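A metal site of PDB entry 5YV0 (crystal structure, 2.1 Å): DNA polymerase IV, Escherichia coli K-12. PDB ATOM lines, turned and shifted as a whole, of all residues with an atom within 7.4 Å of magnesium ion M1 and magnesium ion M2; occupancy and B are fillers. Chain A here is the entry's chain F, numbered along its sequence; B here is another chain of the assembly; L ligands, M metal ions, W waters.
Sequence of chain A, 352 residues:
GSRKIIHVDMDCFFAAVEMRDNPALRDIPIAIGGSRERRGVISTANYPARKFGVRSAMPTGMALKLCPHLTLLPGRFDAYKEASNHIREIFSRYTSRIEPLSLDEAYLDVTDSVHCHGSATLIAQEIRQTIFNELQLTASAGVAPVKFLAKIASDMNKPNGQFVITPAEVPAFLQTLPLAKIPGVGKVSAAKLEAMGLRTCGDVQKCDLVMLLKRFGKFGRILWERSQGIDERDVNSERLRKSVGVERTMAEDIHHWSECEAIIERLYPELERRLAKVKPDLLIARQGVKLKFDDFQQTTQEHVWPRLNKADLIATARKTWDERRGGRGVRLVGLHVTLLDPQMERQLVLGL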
ATOM      1  N   HIS A   7      17.117  -2.324   9.851  1.00  0.00           N
ATOM      2  CA  HIS A   7      16.637  -1.880  11.156  1.00  0.00           C
ATOM      3  C   HIS A   7      16.357  -3.107  12.008  1.00  0.00           C
ATOM      4  O   HIS A   7      15.517  -3.937  11.632  1.00  0.00           O
ATOM      5  CB  HIS A   7      15.387  -1.012  11.015  1.00  0.00           C
ATOM      6  CG  HIS A   7      14.877  -0.510  12.324  1.00  0.00           C
ATOM      7  ND1 HIS A   7      13.801  -1.075  12.970  1.00  0.00           N
ATOM      8  CD2 HIS A   7      15.319   0.500  13.111  1.00  0.00           C
ATOM      9  CE1 HIS A   7      13.590  -0.425  14.104  1.00  0.00           C
ATOM     10  NE2 HIS A   7      14.494   0.546  14.214  1.00  0.00           N
ATOM     11  N   VAL A   8      17.062  -3.228  13.138  1.00  0.00           N
ATOM     12  CA  VAL A   8      16.893  -4.340  14.081  1.00  0.00           C
ATOM     13  C   VAL A   8      16.135  -3.816  15.289  1.00  0.00           C
ATOM     14  O   VAL A   8      16.437  -2.732  15.789  1.00  0.00           O
ATOM     15  CB  VAL A   8      18.244  -4.935  14.499  1.00  0.00           C
ATOM     16  CG1 VAL A   8      18.036  -6.106  15.462  1.00  0.00           C
ATOM     17  CG2 VAL A   8      19.071  -5.359  13.261  1.00  0.00           C
ATOM     18  N   ASP A   9      15.166  -4.606  15.767  1.00  0.00           N
ATOM     19  CA  ASP A   9      14.245  -4.156  16.821  1.00  0.00           C
ATOM     20  C   ASP A   9      13.880  -5.316  17.733  1.00  0.00           C
ATOM     21  O   ASP A   9      13.296  -6.290  17.273  1.00  0.00           O
ATOM     22  CB  ASP A   9      12.975  -3.565  16.202  1.00  0.00           C
ATOM     23  CG  ASP A   9      12.190  -2.725  17.201  1.00  0.00           C
ATOM     24  OD1 ASP A   9      12.738  -2.373  18.261  1.00  0.00           O
ATOM     25  OD2 ASP A   9      11.021  -2.384  16.895  1.00  0.00           O
ATOM     26  N   MET A  10      14.184  -5.188  19.030  1.00  0.00           N
ATOM     27  CA  MET A  10      13.867  -6.257  19.987  1.00  0.00           C
ATOM     28  C   MET A  10      12.362  -6.366  20.177  1.00  0.00           C
ATOM     29  O   MET A  10      11.646  -5.366  20.138  1.00  0.00           O
ATOM     30  CB  MET A  10      14.542  -6.014  21.330  1.00  0.00           C
ATOM     31  CG  MET A  10      16.049  -5.902  21.274  1.00  0.00           C
ATOM     32  SD  MET A  10      16.902  -7.333  20.628  1.00  0.00           S
ATOM     33  CE  MET A  10      16.647  -8.514  21.944  1.00  0.00           C
ATOM     34  N   ASP A  11      11.877  -7.608  20.336  1.00  0.00           N
ATOM     35  CA  ASP A  11      10.455  -7.861  20.554  1.00  0.00           C
ATOM     36  C   ASP A  11      10.089  -7.673  22.032  1.00  0.00           C
ATOM     37  O   ASP A  11      10.734  -8.262  22.905  1.00  0.00           O
ATOM     38  CB  ASP A  11      10.083  -9.289  20.139  1.00  0.00           C
ATOM     39  CG  ASP A  11      10.417  -9.594  18.685  1.00  0.00           C
ATOM     40  OD1 ASP A  11      10.070  -8.792  17.788  1.00  0.00           O
ATOM     41  OD2 ASP A  11      11.008 -10.671  18.444  1.00  0.00           O
ATOM     42  N   CYS A  12       9.043  -6.893  22.297  1.00  0.00           N
ATOM     43  CA  CYS A  12       8.500  -6.653  23.643  1.00  0.00           C
ATOM     44  C   CYS A  12       9.627  -6.487  24.663  1.00  0.00           C
ATOM     45  O   CYS A  12       9.647  -7.142  25.713  1.00  0.00           O
ATOM     46  CB  CYS A  12       7.533  -7.758  24.054  1.00  0.00           C
ATOM     47  SG  CYS A  12       6.134  -7.862  22.912  1.00  0.00           S
ATOM     48  N   PHE A  13      10.576  -5.597  24.321  1.00  0.00           N
ATOM     49  CA  PHE A  13      11.903  -5.619  24.909  1.00  0.00           C
ATOM     50  C   PHE A  13      11.899  -5.773  26.434  1.00  0.00           C
ATOM     51  O   PHE A  13      12.448  -6.754  26.966  1.00  0.00           O
ATOM     52  CB  PHE A  13      12.667  -4.355  24.497  1.00  0.00           C
ATOM     53  CG  PHE A  13      14.077  -4.339  24.989  1.00  0.00           C
ATOM     54  CD1 PHE A  13      14.854  -5.485  24.869  1.00  0.00           C
ATOM     55  CD2 PHE A  13      14.610  -3.220  25.597  1.00  0.00           C
ATOM     56  CE1 PHE A  13      16.146  -5.493  25.342  1.00  0.00           C
ATOM     57  CE2 PHE A  13      15.906  -3.211  26.084  1.00  0.00           C
ATOM     58  CZ  PHE A  13      16.692  -4.339  25.954  1.00  0.00           C
ATOM     59  N   PHE A  14      11.350  -4.795  27.167  1.00  0.00           N
ATOM     60  CA  PHE A  14      11.430  -4.882  28.627  1.00  0.00           C
ATOM     61  C   PHE A  14      10.757  -6.159  29.128  1.00  0.00           C
ATOM     62  O   PHE A  14      11.281  -6.832  30.033  1.00  0.00           O
ATOM     63  CB  PHE A  14      10.770  -3.691  29.328  1.00  0.00           C
ATOM     64  CG  PHE A  14      11.459  -2.365  29.153  1.00  0.00           C
ATOM     65  CD1 PHE A  14      12.567  -2.217  28.330  1.00  0.00           C
ATOM     66  CD2 PHE A  14      10.986  -1.240  29.825  1.00  0.00           C
ATOM     67  CE1 PHE A  14      13.169  -0.961  28.161  1.00  0.00           C
ATOM     68  CE2 PHE A  14      11.570  -0.002  29.677  1.00  0.00           C
ATOM     69  CZ  PHE A  14      12.686   0.146  28.844  1.00  0.00           C
ATOM     70  N   THR A  44       5.536  -1.286  28.434  1.00  0.00           N
ATOM     71  CA  THR A  44       5.298  -2.287  27.412  1.00  0.00           C
ATOM     72  C   THR A  44       4.687  -3.492  28.109  1.00  0.00           C
ATOM     73  O   THR A  44       4.631  -3.570  29.340  1.00  0.00           O
ATOM     74  CB  THR A  44       6.576  -2.658  26.670  1.00  0.00           C
ATOM     75  OG1 THR A  44       6.258  -3.426  25.523  1.00  0.00           O
ATOM     76  CG2 THR A  44       7.488  -3.452  27.589  1.00  0.00           C
ATOM     77  N   ARG A  50      -1.109  -8.114  25.641  1.00  0.00           N
ATOM     78  CA  ARG A  50      -1.571  -7.393  24.446  1.00  0.00           C
ATOM     79  C   ARG A  50      -2.831  -7.999  23.845  1.00  0.00           C
ATOM     80  O   ARG A  50      -3.638  -7.286  23.248  1.00  0.00           O
ATOM     81  CB  ARG A  50      -0.482  -7.400  23.357  1.00  0.00           C
ATOM     82  CG  ARG A  50       0.748  -6.616  23.732  1.00  0.00           C
ATOM     83  CD  ARG A  50       1.841  -6.803  22.669  1.00  0.00           C
ATOM     84  NE  ARG A  50       3.054  -6.095  23.055  1.00  0.00           N
ATOM     85  CZ  ARG A  50       3.228  -4.790  22.938  1.00  0.00           C
ATOM     86  NH1 ARG A  50       2.261  -4.041  22.420  1.00  0.00           N
ATOM     87  NH2 ARG A  50       4.353  -4.227  23.345  1.00  0.00           N
ATOM     88  N   LEU A 101      18.821   3.956  18.020  1.00  0.00           N
ATOM     89  CA  LEU A 101      17.723   4.905  18.172  1.00  0.00           C
ATOM     90  C   LEU A 101      17.128   4.901  19.576  1.00  0.00           C
ATOM     91  O   LEU A 101      16.431   5.858  19.926  1.00  0.00           O
ATOM     92  CB  LEU A 101      16.609   4.612  17.168  1.00  0.00           C
ATOM     93  CG  LEU A 101      17.151   4.506  15.743  1.00  0.00           C
ATOM     94  CD1 LEU A 101      16.135   3.867  14.810  1.00  0.00           C
ATOM     95  CD2 LEU A 101      17.538   5.905  15.262  1.00  0.00           C
ATOM     96  N   SER A 102      17.364   3.857  20.357  1.00  0.00           N
ATOM     97  CA  SER A 102      16.866   3.660  21.716  1.00  0.00           C
ATOM     98  C   SER A 102      17.641   2.457  22.247  1.00  0.00           C
ATOM     99  O   SER A 102      18.548   1.951  21.571  1.00  0.00           O
ATOM    100  CB  SER A 102      15.351   3.462  21.743  1.00  0.00           C
ATOM    101  OG  SER A 102      14.957   2.313  21.011  1.00  0.00           O
ATOM    102  N   LEU A 103      17.299   1.994  23.449  1.00  0.00           N
ATOM    103  CA  LEU A 103      18.000   0.825  23.992  1.00  0.00           C
ATOM    104  C   LEU A 103      17.962  -0.358  23.024  1.00  0.00           C
ATOM    105  O   LEU A 103      18.974  -1.036  22.817  1.00  0.00           O
ATOM    106  CB  LEU A 103      17.387   0.412  25.327  1.00  0.00           C
ATOM    107  CG  LEU A 103      17.665   1.353  26.484  1.00  0.00           C
ATOM    108  CD1 LEU A 103      17.085   0.746  27.736  1.00  0.00           C
ATOM    109  CD2 LEU A 103      19.157   1.581  26.615  1.00  0.00           C
ATOM    110  N   ASP A 104      16.801  -0.610  22.411  1.00  0.00           N
ATOM    111  CA  ASP A 104      16.493  -1.918  21.841  1.00  0.00           C
ATOM    112  C   ASP A 104      16.485  -1.949  20.316  1.00  0.00           C
ATOM    113  O   ASP A 104      16.024  -2.947  19.738  1.00  0.00           O
ATOM    114  CB  ASP A 104      15.146  -2.426  22.395  1.00  0.00           C
ATOM    115  CG  ASP A 104      13.961  -2.031  21.534  1.00  0.00           C
ATOM    116  OD1 ASP A 104      13.923  -0.887  21.030  1.00  0.00           O
ATOM    117  OD2 ASP A 104      13.074  -2.878  21.331  1.00  0.00           O
ATOM    118  N   GLU A 105      16.984  -0.908  19.647  1.00  0.00           N
ATOM    119  CA  GLU A 105      16.902  -0.879  18.202  1.00  0.00           C
ATOM    120  C   GLU A 105      18.012  -0.009  17.624  1.00  0.00           C
ATOM    121  O   GLU A 105      18.554   0.866  18.315  1.00  0.00           O
ATOM    122  CB  GLU A 105      15.511  -0.404  17.735  1.00  0.00           C
ATOM    123  CG  GLU A 105      15.234   1.074  17.815  1.00  0.00           C
ATOM    124  CD  GLU A 105      13.806   1.414  17.396  1.00  0.00           C
ATOM    125  OE1 GLU A 105      12.851   0.932  18.047  1.00  0.00           O
ATOM    126  OE2 GLU A 105      13.611   2.175  16.423  1.00  0.00           O
ATOM    127  N   ALA A 106      18.377  -0.296  16.385  1.00  0.00           N
ATOM    128  CA  ALA A 106      19.407   0.449  15.668  1.00  0.00           C
ATOM    129  C   ALA A 106      19.170   0.338  14.176  1.00  0.00           C
ATOM    130  O   ALA A 106      18.596  -0.641  13.697  1.00  0.00           O
ATOM    131  CB  ALA A 106      20.816  -0.068  15.971  1.00  0.00           C
ATOM    132  N   LYS A 151      12.642   0.731   8.864  1.00  0.00           N
ATOM    133  CA  LYS A 151      12.041   0.769  10.188  1.00  0.00           C
ATOM    134  C   LYS A 151      10.574   0.337  10.126  1.00  0.00           C
ATOM    135  O   LYS A 151      10.099  -0.402  10.988  1.00  0.00           O
ATOM    136  CB  LYS A 151      12.201   2.171  10.811  1.00  0.00           C
ATOM    137  CG  LYS A 151      11.482   2.310  12.178  1.00  0.00           C
ATOM    138  CD  LYS A 151      12.100   3.502  12.975  1.00  0.00           C
ATOM    139  CE  LYS A 151      11.264   3.827  14.229  1.00  0.00           C
ATOM    140  NZ  LYS A 151      11.177   2.720  15.233  1.00  0.00           N
ATOM    141  N   ASP A 155       8.592  -3.817  11.683  1.00  0.00           N
ATOM    142  CA  ASP A 155       7.336  -4.028  12.384  1.00  0.00           C
ATOM    143  C   ASP A 155       6.442  -5.071  11.737  1.00  0.00           C
ATOM    144  O   ASP A 155       5.568  -5.628  12.419  1.00  0.00           O
ATOM    145  CB  ASP A 155       6.556  -2.725  12.470  1.00  0.00           C
ATOM    146  CG  ASP A 155       6.658  -2.087  13.809  1.00  0.00           C
ATOM    147  OD1 ASP A 155       7.573  -2.479  14.577  1.00  0.00           O
ATOM    148  OD2 ASP A 155       5.827  -1.201  14.107  1.00  0.00           O
ATOM    149  N   LYS A 158       6.899  -9.015  12.917  1.00  0.00           N
ATOM    150  CA  LYS A 158       7.294  -9.309  14.286  1.00  0.00           C
ATOM    151  C   LYS A 158       6.162 -10.073  15.008  1.00  0.00           C
ATOM    152  O   LYS A 158       5.010 -10.000  14.593  1.00  0.00           O
ATOM    153  CB  LYS A 158       7.756  -8.026  15.027  1.00  0.00           C
ATOM    154  CG  LYS A 158       6.742  -7.020  15.488  1.00  0.00           C
ATOM    155  CD  LYS A 158       7.422  -6.035  16.499  1.00  0.00           C
ATOM    156  CE  LYS A 158       8.906  -5.702  16.141  1.00  0.00           C
ATOM    157  NZ  LYS A 158       9.936  -6.002  17.237  1.00  0.00           N
ATOM    158  P    DC B  18       8.910   4.580  17.732  1.00  0.00           P
ATOM    159  OP1  DC B  18       9.305   3.559  16.752  1.00  0.00           O
ATOM    160  OP2  DC B  18       7.478   4.769  18.052  1.00  0.00           O
ATOM    161  O5'  DC B  18       9.690   4.241  19.086  1.00  0.00           O
ATOM    162  C5'  DC B  18      11.073   3.889  19.027  1.00  0.00           C
ATOM    163  C4'  DC B  18      11.594   3.608  20.413  1.00  0.00           C
ATOM    164  O4'  DC B  18      11.551   4.836  21.200  1.00  0.00           O
ATOM    165  C3'  DC B  18      10.767   2.622  21.211  1.00  0.00           C
ATOM    166  O3'  DC B  18      11.111   1.290  20.887  1.00  0.00           O
ATOM    167  C2'  DC B  18      11.142   2.985  22.645  1.00  0.00           C
ATOM    168  C1'  DC B  18      11.287   4.520  22.550  1.00  0.00           C
ATOM    169  N1   DC B  18      10.087   5.282  22.981  1.00  0.00           N
ATOM    170  C2   DC B  18       9.949   5.587  24.315  1.00  0.00           C
ATOM    171  O2   DC B  18      10.810   5.171  25.101  1.00  0.00           O
ATOM    172  N3   DC B  18       8.868   6.322  24.726  1.00  0.00           N
ATOM    173  C4   DC B  18       7.973   6.729  23.817  1.00  0.00           C
ATOM    174  N4   DC B  18       6.930   7.441  24.251  1.00  0.00           N
ATOM    175  C5   DC B  18       8.091   6.396  22.437  1.00  0.00           C
ATOM    176  C6   DC B  18       9.165   5.700  22.058  1.00  0.00           C
ATOM    177  P    DT B  19      10.036   0.096  21.079  1.00  0.00           P
ATOM    178  OP1  DT B  19      10.543  -1.132  20.385  1.00  0.00           O
ATOM    179  OP2  DT B  19       8.707   0.655  20.727  1.00  0.00           O
ATOM    180  O5'  DT B  19      10.037  -0.146  22.653  1.00  0.00           O
ATOM    181  C5'  DT B  19      11.218  -0.635  23.320  1.00  0.00           C
ATOM    182  C4'  DT B  19      11.053  -0.519  24.838  1.00  0.00           C
ATOM    183  O4'  DT B  19      10.946   0.879  25.202  1.00  0.00           O
ATOM    184  C3'  DT B  19       9.759  -1.149  25.387  1.00  0.00           C
ATOM    185  O3'  DT B  19       9.932  -2.516  25.652  1.00  0.00           O
ATOM    186  C2'  DT B  19       9.572  -0.393  26.686  1.00  0.00           C
ATOM    187  C1'  DT B  19      10.042   1.022  26.297  1.00  0.00           C
ATOM    188  N1   DT B  19       8.903   1.932  25.916  1.00  0.00           N
ATOM    189  C2   DT B  19       8.406   2.773  26.875  1.00  0.00           C
ATOM    190  O2   DT B  19       8.854   2.821  27.986  1.00  0.00           O
ATOM    191  N3   DT B  19       7.360   3.552  26.467  1.00  0.00           N
ATOM    192  C4   DT B  19       6.772   3.573  25.219  1.00  0.00           C
ATOM    193  O4   DT B  19       5.816   4.310  24.943  1.00  0.00           O
ATOM    194  C5   DT B  19       7.320   2.636  24.262  1.00  0.00           C
ATOM    195  C7   DT B  19       6.743   2.540  22.851  1.00  0.00           C
ATOM    196  C6   DT B  19       8.353   1.868  24.660  1.00  0.00           C
HETATM  197  P1  LIG L   1       8.360  -3.237  22.568  1.00  0.00           P
HETATM  198  O1  LIG L   1       9.767  -3.616  22.200  1.00  0.00           O
HETATM  199  O2  LIG L   1       8.218  -3.265  24.054  1.00  0.00           O
HETATM  200  O3  LIG L   1       7.929  -1.967  21.851  1.00  0.00           O
HETATM  201  O4  LIG L   1       7.312  -4.306  22.349  1.00  0.00           O
HETATM  202 MG    MG M   1      12.504  -0.485  19.516  1.00  0.00          MG
HETATM  203 MG    MG M   2      10.953  -3.210  20.323  1.00  0.00          MG
HETATM  204  O   HOH W   1      10.522   0.538  17.334  1.00  0.00           O
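Water W1 lies within hydrogen-bond range of the side-chain carboxylate (OD2) of Asp 9 (3.0 Å), the side-chain amino group (NZ) of Lys 151 (3.1 Å) and OP1 of DC 18 of chain B (3.3 Å).
Magnesium ion M1 is bound by the side-chain carboxylate of Glu 105 (2.1 Å), the side-chain carboxylate of Asp 104 (2.1 Å), OP1 of DT 19 of chain B (2.2 Å) and the side-chain carboxylate of Asp 9 (2.3 Å). Slightly farther from magnesium ion M1 lies O3' of DC 18 of chain B (2.6 Å).
Four residues have an atom within 4 Å of magnesium ion M2: Asp 9, Met 10, Asp 104 and DT 19 of chain B. Along chain A the residues within 4 Å of magnesium ion M2 span positions 9 to 104.
Magnesium ion M2 is bound by OP1 of DT 19 of chain B (2.1 Å), an oxygen (O1) of the ligand (2.3 Å), the backbone carbonyl oxygen (O) of Met 10 (2.3 Å) and the side-chain carboxylate (OD2) of Asp 104 (2.4 Å). Magnesium ion M2 has four donor atoms within binding distance.
The side-chain carboxylate (OD1) of Asp 104 lies close to the side-chain hydroxyl (OG) of Ser 102 (3.4 Å). The side-chain carboxylate (OE2) of Glu 105 is in salt-bridge range of the side-chain amino group (NZ) of Lys 151 (2.8 Å). The backbone carbonyl oxygen of Met 10 sits close to the side-chain amino group of Lys 158. The side-chain carboxylate (OD2) of Asp 9 lies within salt-bridge range of the side-chain amino group (NZ) of Lys 158, 3.8 Å away. OP1 of DC 18 of chain B is in salt-bridge range of the side-chain amino group (NZ) of Lys 151, at 2.6 Å. The backbone NH (N) of Phe 13 sits at hydrogen-bond distance from O3' of DT 19 of chain B (3.4 Å). The side-chain carboxylate (OE2) of Glu 105 is in hydrogen-bond range of a ring nitrogen (NE2) of His 7, 2.9 Å away. O3' of DT 19 of chain B is in hydrogen-bond range of the backbone NH (N) of Phe 14 (3.1 Å).
Five residues have an atom within 4 Å of magnesium ion M1: Asp 9, Asp 104, Glu 105, DC 18 of chain B and DT 19 of chain B. Along chain A the residues within 4 Å of magnesium ion M1 span positions 9 to 105.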
